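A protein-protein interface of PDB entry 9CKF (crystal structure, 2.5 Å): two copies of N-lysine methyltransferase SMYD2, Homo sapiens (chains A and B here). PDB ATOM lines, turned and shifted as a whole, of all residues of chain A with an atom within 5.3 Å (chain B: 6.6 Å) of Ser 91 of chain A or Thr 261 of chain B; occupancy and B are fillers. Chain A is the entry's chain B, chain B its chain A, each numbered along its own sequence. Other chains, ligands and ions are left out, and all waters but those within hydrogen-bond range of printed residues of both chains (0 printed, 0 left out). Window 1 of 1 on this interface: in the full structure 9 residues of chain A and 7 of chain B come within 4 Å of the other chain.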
ATOM      1  N   HIS A  86      -0.721 -21.701   3.855  1.00  0.00           N
ATOM      2  CA  HIS A  86      -0.309 -21.001   2.644  1.00  0.00           C
ATOM      3  C   HIS A  86       0.067 -19.551   2.918  1.00  0.00           C
ATOM      4  O   HIS A  86       0.903 -18.988   2.202  1.00  0.00           O
ATOM      5  CB  HIS A  86      -1.423 -21.072   1.599  1.00  0.00           C
ATOM      6  CG  HIS A  86      -1.108 -20.344   0.333  1.00  0.00           C
ATOM      7  ND1 HIS A  86       0.092 -20.488  -0.329  1.00  0.00           N
ATOM      8  CD2 HIS A  86      -1.836 -19.467  -0.397  1.00  0.00           C
ATOM      9  CE1 HIS A  86       0.091 -19.727  -1.409  1.00  0.00           C
ATOM     10  NE2 HIS A  86      -1.069 -19.100  -1.475  1.00  0.00           N
ATOM     11  N   LYS A  87      -0.522 -18.933   3.946  1.00  0.00           N
ATOM     12  CA  LYS A  87      -0.225 -17.534   4.233  1.00  0.00           C
ATOM     13  C   LYS A  87       1.225 -17.323   4.641  1.00  0.00           C
ATOM     14  O   LYS A  87       1.708 -16.186   4.608  1.00  0.00           O
ATOM     15  CB  LYS A  87      -1.159 -16.995   5.319  1.00  0.00           C
ATOM     16  CG  LYS A  87      -1.047 -17.683   6.665  1.00  0.00           C
ATOM     17  CD  LYS A  87      -2.151 -17.200   7.592  1.00  0.00           C
ATOM     18  CE  LYS A  87      -2.047 -17.820   8.973  1.00  0.00           C
ATOM     19  NZ  LYS A  87      -3.195 -17.413   9.832  1.00  0.00           N
ATOM     20  N   GLU A  89       3.696 -18.307   2.912  1.00  0.00           N
ATOM     21  CA  GLU A  89       4.438 -18.123   1.677  1.00  0.00           C
ATOM     22  C   GLU A  89       3.736 -17.240   0.656  1.00  0.00           C
ATOM     23  O   GLU A  89       4.416 -16.686  -0.212  1.00  0.00           O
ATOM     24  CB  GLU A  89       4.729 -19.485   1.024  1.00  0.00           C
ATOM     25  CG  GLU A  89       5.342 -20.502   1.974  1.00  0.00           C
ATOM     26  CD  GLU A  89       5.605 -21.839   1.311  1.00  0.00           C
ATOM     27  OE1 GLU A  89       4.778 -22.258   0.474  1.00  0.00           O
ATOM     28  OE2 GLU A  89       6.635 -22.469   1.631  1.00  0.00           O
ATOM     29  N   CYS A  90       2.411 -17.087   0.740  1.00  0.00           N
ATOM     30  CA  CYS A  90       1.670 -16.327  -0.264  1.00  0.00           C
ATOM     31  C   CYS A  90       2.226 -14.914  -0.416  1.00  0.00           C
ATOM     32  O   CYS A  90       2.609 -14.496  -1.515  1.00  0.00           O
ATOM     33  CB  CYS A  90       0.184 -16.288   0.100  1.00  0.00           C
ATOM     34  SG  CYS A  90      -0.851 -15.436  -1.110  1.00  0.00           S
ATOM     35  N   SER A  91       2.272 -14.157   0.686  1.00  0.00           N
ATOM     36  CA  SER A  91       2.791 -12.793   0.603  1.00  0.00           C
ATOM     37  C   SER A  91       4.286 -12.754   0.296  1.00  0.00           C
ATOM     38  O   SER A  91       4.681 -12.014  -0.622  1.00  0.00           O
ATOM     39  CB  SER A  91       2.454 -12.027   1.885  1.00  0.00           C
ATOM     40  OG  SER A  91       2.921 -10.691   1.810  1.00  0.00           O
ATOM     41  N   PRO A  92       5.160 -13.505   0.983  1.00  0.00           N
ATOM     42  CA  PRO A  92       6.597 -13.388   0.679  1.00  0.00           C
ATOM     43  C   PRO A  92       6.968 -13.822  -0.726  1.00  0.00           C
ATOM     44  O   PRO A  92       7.995 -13.370  -1.244  1.00  0.00           O
ATOM     45  CB  PRO A  92       7.256 -14.289   1.732  1.00  0.00           C
ATOM     46  CG  PRO A  92       6.270 -14.375   2.829  1.00  0.00           C
ATOM     47  CD  PRO A  92       4.934 -14.366   2.158  1.00  0.00           C
ATOM     48  N   MET A  93       6.184 -14.697  -1.359  1.00  0.00           N
ATOM     49  CA  MET A  93       6.524 -15.114  -2.716  1.00  0.00           C
ATOM     50  C   MET A  93       6.429 -13.954  -3.699  1.00  0.00           C
ATOM     51  O   MET A  93       7.203 -13.893  -4.661  1.00  0.00           O
ATOM     52  CB  MET A  93       5.623 -16.264  -3.160  1.00  0.00           C
ATOM     53  CG  MET A  93       6.038 -17.617  -2.609  1.00  0.00           C
ATOM     54  SD  MET A  93       4.998 -18.950  -3.221  1.00  0.00           S
ATOM     55  CE  MET A  93       5.350 -18.827  -4.962  1.00  0.00           C
ATOM     56  N   VAL A  94       5.503 -13.023  -3.471  1.00  0.00           N
ATOM     57  CA  VAL A  94       5.389 -11.865  -4.351  1.00  0.00           C
ATOM     58  C   VAL A  94       6.388 -10.785  -3.953  1.00  0.00           C
ATOM     59  O   VAL A  94       6.969 -10.114  -4.813  1.00  0.00           O
ATOM     60  CB  VAL A  94       3.945 -11.335  -4.336  1.00  0.00           C
ATOM     61  CG1 VAL A  94       3.778 -10.215  -5.351  1.00  0.00           C
ATOM     62  CG2 VAL A  94       2.966 -12.467  -4.614  1.00  0.00           C
ATOM     63  N   VAL A  95       6.618 -10.616  -2.649  1.00  0.00           N
ATOM     64  CA  VAL A  95       7.533  -9.581  -2.175  1.00  0.00           C
ATOM     65  C   VAL A  95       8.970  -9.915  -2.561  1.00  0.00           C
ATOM     66  O   VAL A  95       9.706  -9.063  -3.073  1.00  0.00           O
ATOM     67  CB  VAL A  95       7.384  -9.395  -0.655  1.00  0.00           C
ATOM     68  CG1 VAL A  95       8.428  -8.424  -0.134  1.00  0.00           C
ATOM     69  CG2 VAL A  95       5.982  -8.909  -0.316  1.00  0.00           C
ATOM     70  N   PHE A  96       9.390 -11.160  -2.324  1.00  0.00           N
ATOM     71  CA  PHE A  96      10.752 -11.562  -2.661  1.00  0.00           C
ATOM     72  C   PHE A  96      10.937 -11.776  -4.159  1.00  0.00           C
ATOM     73  O   PHE A  96      12.042 -11.574  -4.675  1.00  0.00           O
ATOM     74  CB  PHE A  96      11.132 -12.838  -1.908  1.00  0.00           C
ATOM     75  CG  PHE A  96      11.415 -12.627  -0.446  1.00  0.00           C
ATOM     76  CD1 PHE A  96      10.402 -12.727   0.493  1.00  0.00           C
ATOM     77  CD2 PHE A  96      12.701 -12.345  -0.012  1.00  0.00           C
ATOM     78  CE1 PHE A  96      10.662 -12.541   1.838  1.00  0.00           C
ATOM     79  CE2 PHE A  96      12.969 -12.159   1.330  1.00  0.00           C
ATOM     80  CZ  PHE A  96      11.949 -12.258   2.257  1.00  0.00           C
ATOM     81  N   ASN B 251      -2.489  -2.921  -2.555  1.00  0.00           N
ATOM     82  CA  ASN B 251      -1.466  -3.857  -2.107  1.00  0.00           C
ATOM     83  C   ASN B 251      -0.241  -3.856  -3.011  1.00  0.00           C
ATOM     84  O   ASN B 251       0.822  -4.317  -2.585  1.00  0.00           O
ATOM     85  CB  ASN B 251      -2.057  -5.260  -2.006  1.00  0.00           C
ATOM     86  CG  ASN B 251      -3.017  -5.395  -0.843  1.00  0.00           C
ATOM     87  OD1 ASN B 251      -2.618  -5.738   0.269  1.00  0.00           O
ATOM     88  ND2 ASN B 251      -4.288  -5.110  -1.090  1.00  0.00           N
ATOM     89  N   LEU B 254       1.796  -1.276  -1.378  1.00  0.00           N
ATOM     90  CA  LEU B 254       2.241  -1.773  -0.081  1.00  0.00           C
ATOM     91  C   LEU B 254       3.375  -2.780  -0.232  1.00  0.00           C
ATOM     92  O   LEU B 254       4.368  -2.717   0.502  1.00  0.00           O
ATOM     93  CB  LEU B 254       1.064  -2.386   0.674  1.00  0.00           C
ATOM     94  CG  LEU B 254      -0.022  -1.392   1.085  1.00  0.00           C
ATOM     95  CD1 LEU B 254      -1.111  -2.083   1.893  1.00  0.00           C
ATOM     96  CD2 LEU B 254       0.574  -0.233   1.868  1.00  0.00           C
ATOM     97  N   ARG B 255       3.246  -3.715  -1.176  1.00  0.00           N
ATOM     98  CA  ARG B 255       4.321  -4.668  -1.429  1.00  0.00           C
ATOM     99  C   ARG B 255       5.560  -3.991  -2.005  1.00  0.00           C
ATOM    100  O   ARG B 255       6.686  -4.413  -1.718  1.00  0.00           O
ATOM    101  CB  ARG B 255       3.833  -5.767  -2.375  1.00  0.00           C
ATOM    102  CG  ARG B 255       2.848  -6.734  -1.743  1.00  0.00           C
ATOM    103  CD  ARG B 255       2.647  -7.978  -2.600  1.00  0.00           C
ATOM    104  NE  ARG B 255       1.867  -7.706  -3.804  1.00  0.00           N
ATOM    105  CZ  ARG B 255       0.555  -7.903  -3.902  1.00  0.00           C
ATOM    106  NH1 ARG B 255      -0.124  -8.376  -2.866  1.00  0.00           N
ATOM    107  NH2 ARG B 255      -0.078  -7.628  -5.034  1.00  0.00           N
ATOM    108  N   PHE B 259       6.922  -3.876   1.545  1.00  0.00           N
ATOM    109  CA  PHE B 259       7.253  -5.302   1.563  1.00  0.00           C
ATOM    110  C   PHE B 259       6.285  -6.098   2.441  1.00  0.00           C
ATOM    111  O   PHE B 259       6.692  -6.873   3.309  1.00  0.00           O
ATOM    112  CB  PHE B 259       8.703  -5.514   2.013  1.00  0.00           C
ATOM    113  CG  PHE B 259       9.708  -4.702   1.237  1.00  0.00           C
ATOM    114  CD1 PHE B 259      10.240  -5.180   0.050  1.00  0.00           C
ATOM    115  CD2 PHE B 259      10.122  -3.460   1.696  1.00  0.00           C
ATOM    116  CE1 PHE B 259      11.165  -4.438  -0.666  1.00  0.00           C
ATOM    117  CE2 PHE B 259      11.044  -2.711   0.985  1.00  0.00           C
ATOM    118  CZ  PHE B 259      11.566  -3.201  -0.199  1.00  0.00           C
ATOM    119  N   PHE B 260       4.988  -5.899   2.210  1.00  0.00           N
ATOM    120  CA  PHE B 260       3.958  -6.674   2.893  1.00  0.00           C
ATOM    121  C   PHE B 260       2.663  -6.559   2.102  1.00  0.00           C
ATOM    122  O   PHE B 260       2.527  -5.707   1.221  1.00  0.00           O
ATOM    123  CB  PHE B 260       3.758  -6.202   4.338  1.00  0.00           C
ATOM    124  CG  PHE B 260       2.862  -5.003   4.471  1.00  0.00           C
ATOM    125  CD1 PHE B 260       3.349  -3.726   4.246  1.00  0.00           C
ATOM    126  CD2 PHE B 260       1.535  -5.149   4.845  1.00  0.00           C
ATOM    127  CE1 PHE B 260       2.527  -2.622   4.374  1.00  0.00           C
ATOM    128  CE2 PHE B 260       0.710  -4.049   4.973  1.00  0.00           C
ATOM    129  CZ  PHE B 260       1.206  -2.785   4.737  1.00  0.00           C
ATOM    130  N   THR B 261       1.712  -7.433   2.423  1.00  0.00           N
ATOM    131  CA  THR B 261       0.382  -7.424   1.821  1.00  0.00           C
ATOM    132  C   THR B 261      -0.654  -7.284   2.923  1.00  0.00           C
ATOM    133  O   THR B 261      -0.699  -8.108   3.843  1.00  0.00           O
ATOM    134  CB  THR B 261       0.121  -8.693   1.010  1.00  0.00           C
ATOM    135  OG1 THR B 261       1.103  -8.809  -0.022  1.00  0.00           O
ATOM    136  CG2 THR B 261      -1.265  -8.650   0.391  1.00  0.00           C
ATOM    137  N   CYS B 262      -1.431  -6.199   2.842  1.00  0.00           N
ATOM    138  CA  CYS B 262      -2.483  -5.877   3.841  1.00  0.00           C
ATOM    139  C   CYS B 262      -3.493  -7.024   3.915  1.00  0.00           C
ATOM    140  O   CYS B 262      -3.862  -7.560   2.850  1.00  0.00           O
ATOM    141  CB  CYS B 262      -3.203  -4.584   3.473  1.00  0.00           C
ATOM    142  SG  CYS B 262      -4.189  -3.898   4.828  1.00  0.00           S
ATOM    143  N   GLU B 263      -3.914  -7.376   5.132  1.00  0.00           N
ATOM    144  CA  GLU B 263      -4.896  -8.472   5.336  1.00  0.00           C
ATOM    145  C   GLU B 263      -5.999  -7.982   6.280  1.00  0.00           C
ATOM    146  O   GLU B 263      -6.339  -8.726   7.221  1.00  0.00           O
ATOM    147  CB  GLU B 263      -4.202  -9.712   5.902  1.00  0.00           C
ATOM    148  CG  GLU B 263      -4.034 -10.827   4.887  1.00  0.00           C
ATOM    149  CD  GLU B 263      -2.930 -11.818   5.210  1.00  0.00           C
ATOM    150  OE1 GLU B 263      -2.718 -12.094   6.408  1.00  0.00           O
ATOM    151  OE2 GLU B 263      -2.285 -12.311   4.264  1.00  0.00           O
ATOM    152  N   CYS B 264      -6.535  -6.779   6.036  1.00  0.00           N
ATOM    153  CA  CYS B 264      -7.595  -6.263   6.889  1.00  0.00           C
ATOM    154  C   CYS B 264      -8.955  -6.688   6.330  1.00  0.00           C
ATOM    155  O   CYS B 264      -9.056  -7.502   5.408  1.00  0.00           O
ATOM    156  CB  CYS B 264      -7.470  -4.750   7.018  1.00  0.00           C
ATOM    157  SG  CYS B 264      -7.722  -3.848   5.471  1.00  0.00           S
ATOM    158  N   CYS B 267      -9.340  -5.590   2.502  1.00  0.00           N
ATOM    159  CA  CYS B 267      -8.413  -6.314   1.586  1.00  0.00           C
ATOM    160  C   CYS B 267      -8.781  -7.795   1.428  1.00  0.00           C
ATOM    161  O   CYS B 267      -8.418  -8.373   0.383  1.00  0.00           O
ATOM    162  CB  CYS B 267      -6.974  -6.202   2.078  1.00  0.00           C
ATOM    163  SG  CYS B 267      -6.176  -4.641   1.622  1.00  0.00           S
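OG1 of Thr 261 of chain B is in hydrogen-bond range of OG of Ser 91 of chain A, 3.2 Å away.
The backbone carbonyl oxygen (O) of Leu 254 of chain B lies within hydrogen-bond range of the backbone NH (N) of Phe 259 of chain B (3.0 Å). The backbone NH of Arg 255 of chain B lies close to the backbone carbonyl oxygen of Phe 260 of chain B (3.2 Å). The guanidinium group of Arg 255 of chain B sits close to the side-chain hydroxyl of Thr 261 of chain B, at 3.1 Å.
Among the printed residues, pairs that only touch across the chains: Val 94 of chain A with Arg 255 of chain B and Val 95 of chain A with Phe 259 of chain B.
His 86 of chain A touches none of the printed residues of chain B. Met 93 of chain A touches none of the printed residues of chain B. Of the printed residues of chain B, Val 94 of chain A touches Arg 255 (3.5 Å). Of the printed residues of chain A, Arg 255 of chain B touches Val 94. Thr 261 of chain B touches just one residue of chain A: Ser 91 (3.2 Å). The nearest residue of chain B that does not touch Ser 91 of chain A is Phe 260 of chain B (4.2 Å).
Of the 10 printed residues of chain A, 3 touch a printed residue of chain B. Printed residues of chain A that touch a printed residue of chain B: Ser 91, Val 94 and Val 95. Hydrophobic or aromatic side chains of chain B within 4 Å of the printed part of chain A: Phe 259. Among the printed residues, no Asp or Glu carboxylate lies within 4 Å of a Lys or Arg side-chain nitrogen of the other chain.
No position is printed for both chains. Of the 3 pairs that touch across the chains among the printed residues, none has its exchanged pair printed and touching as well.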
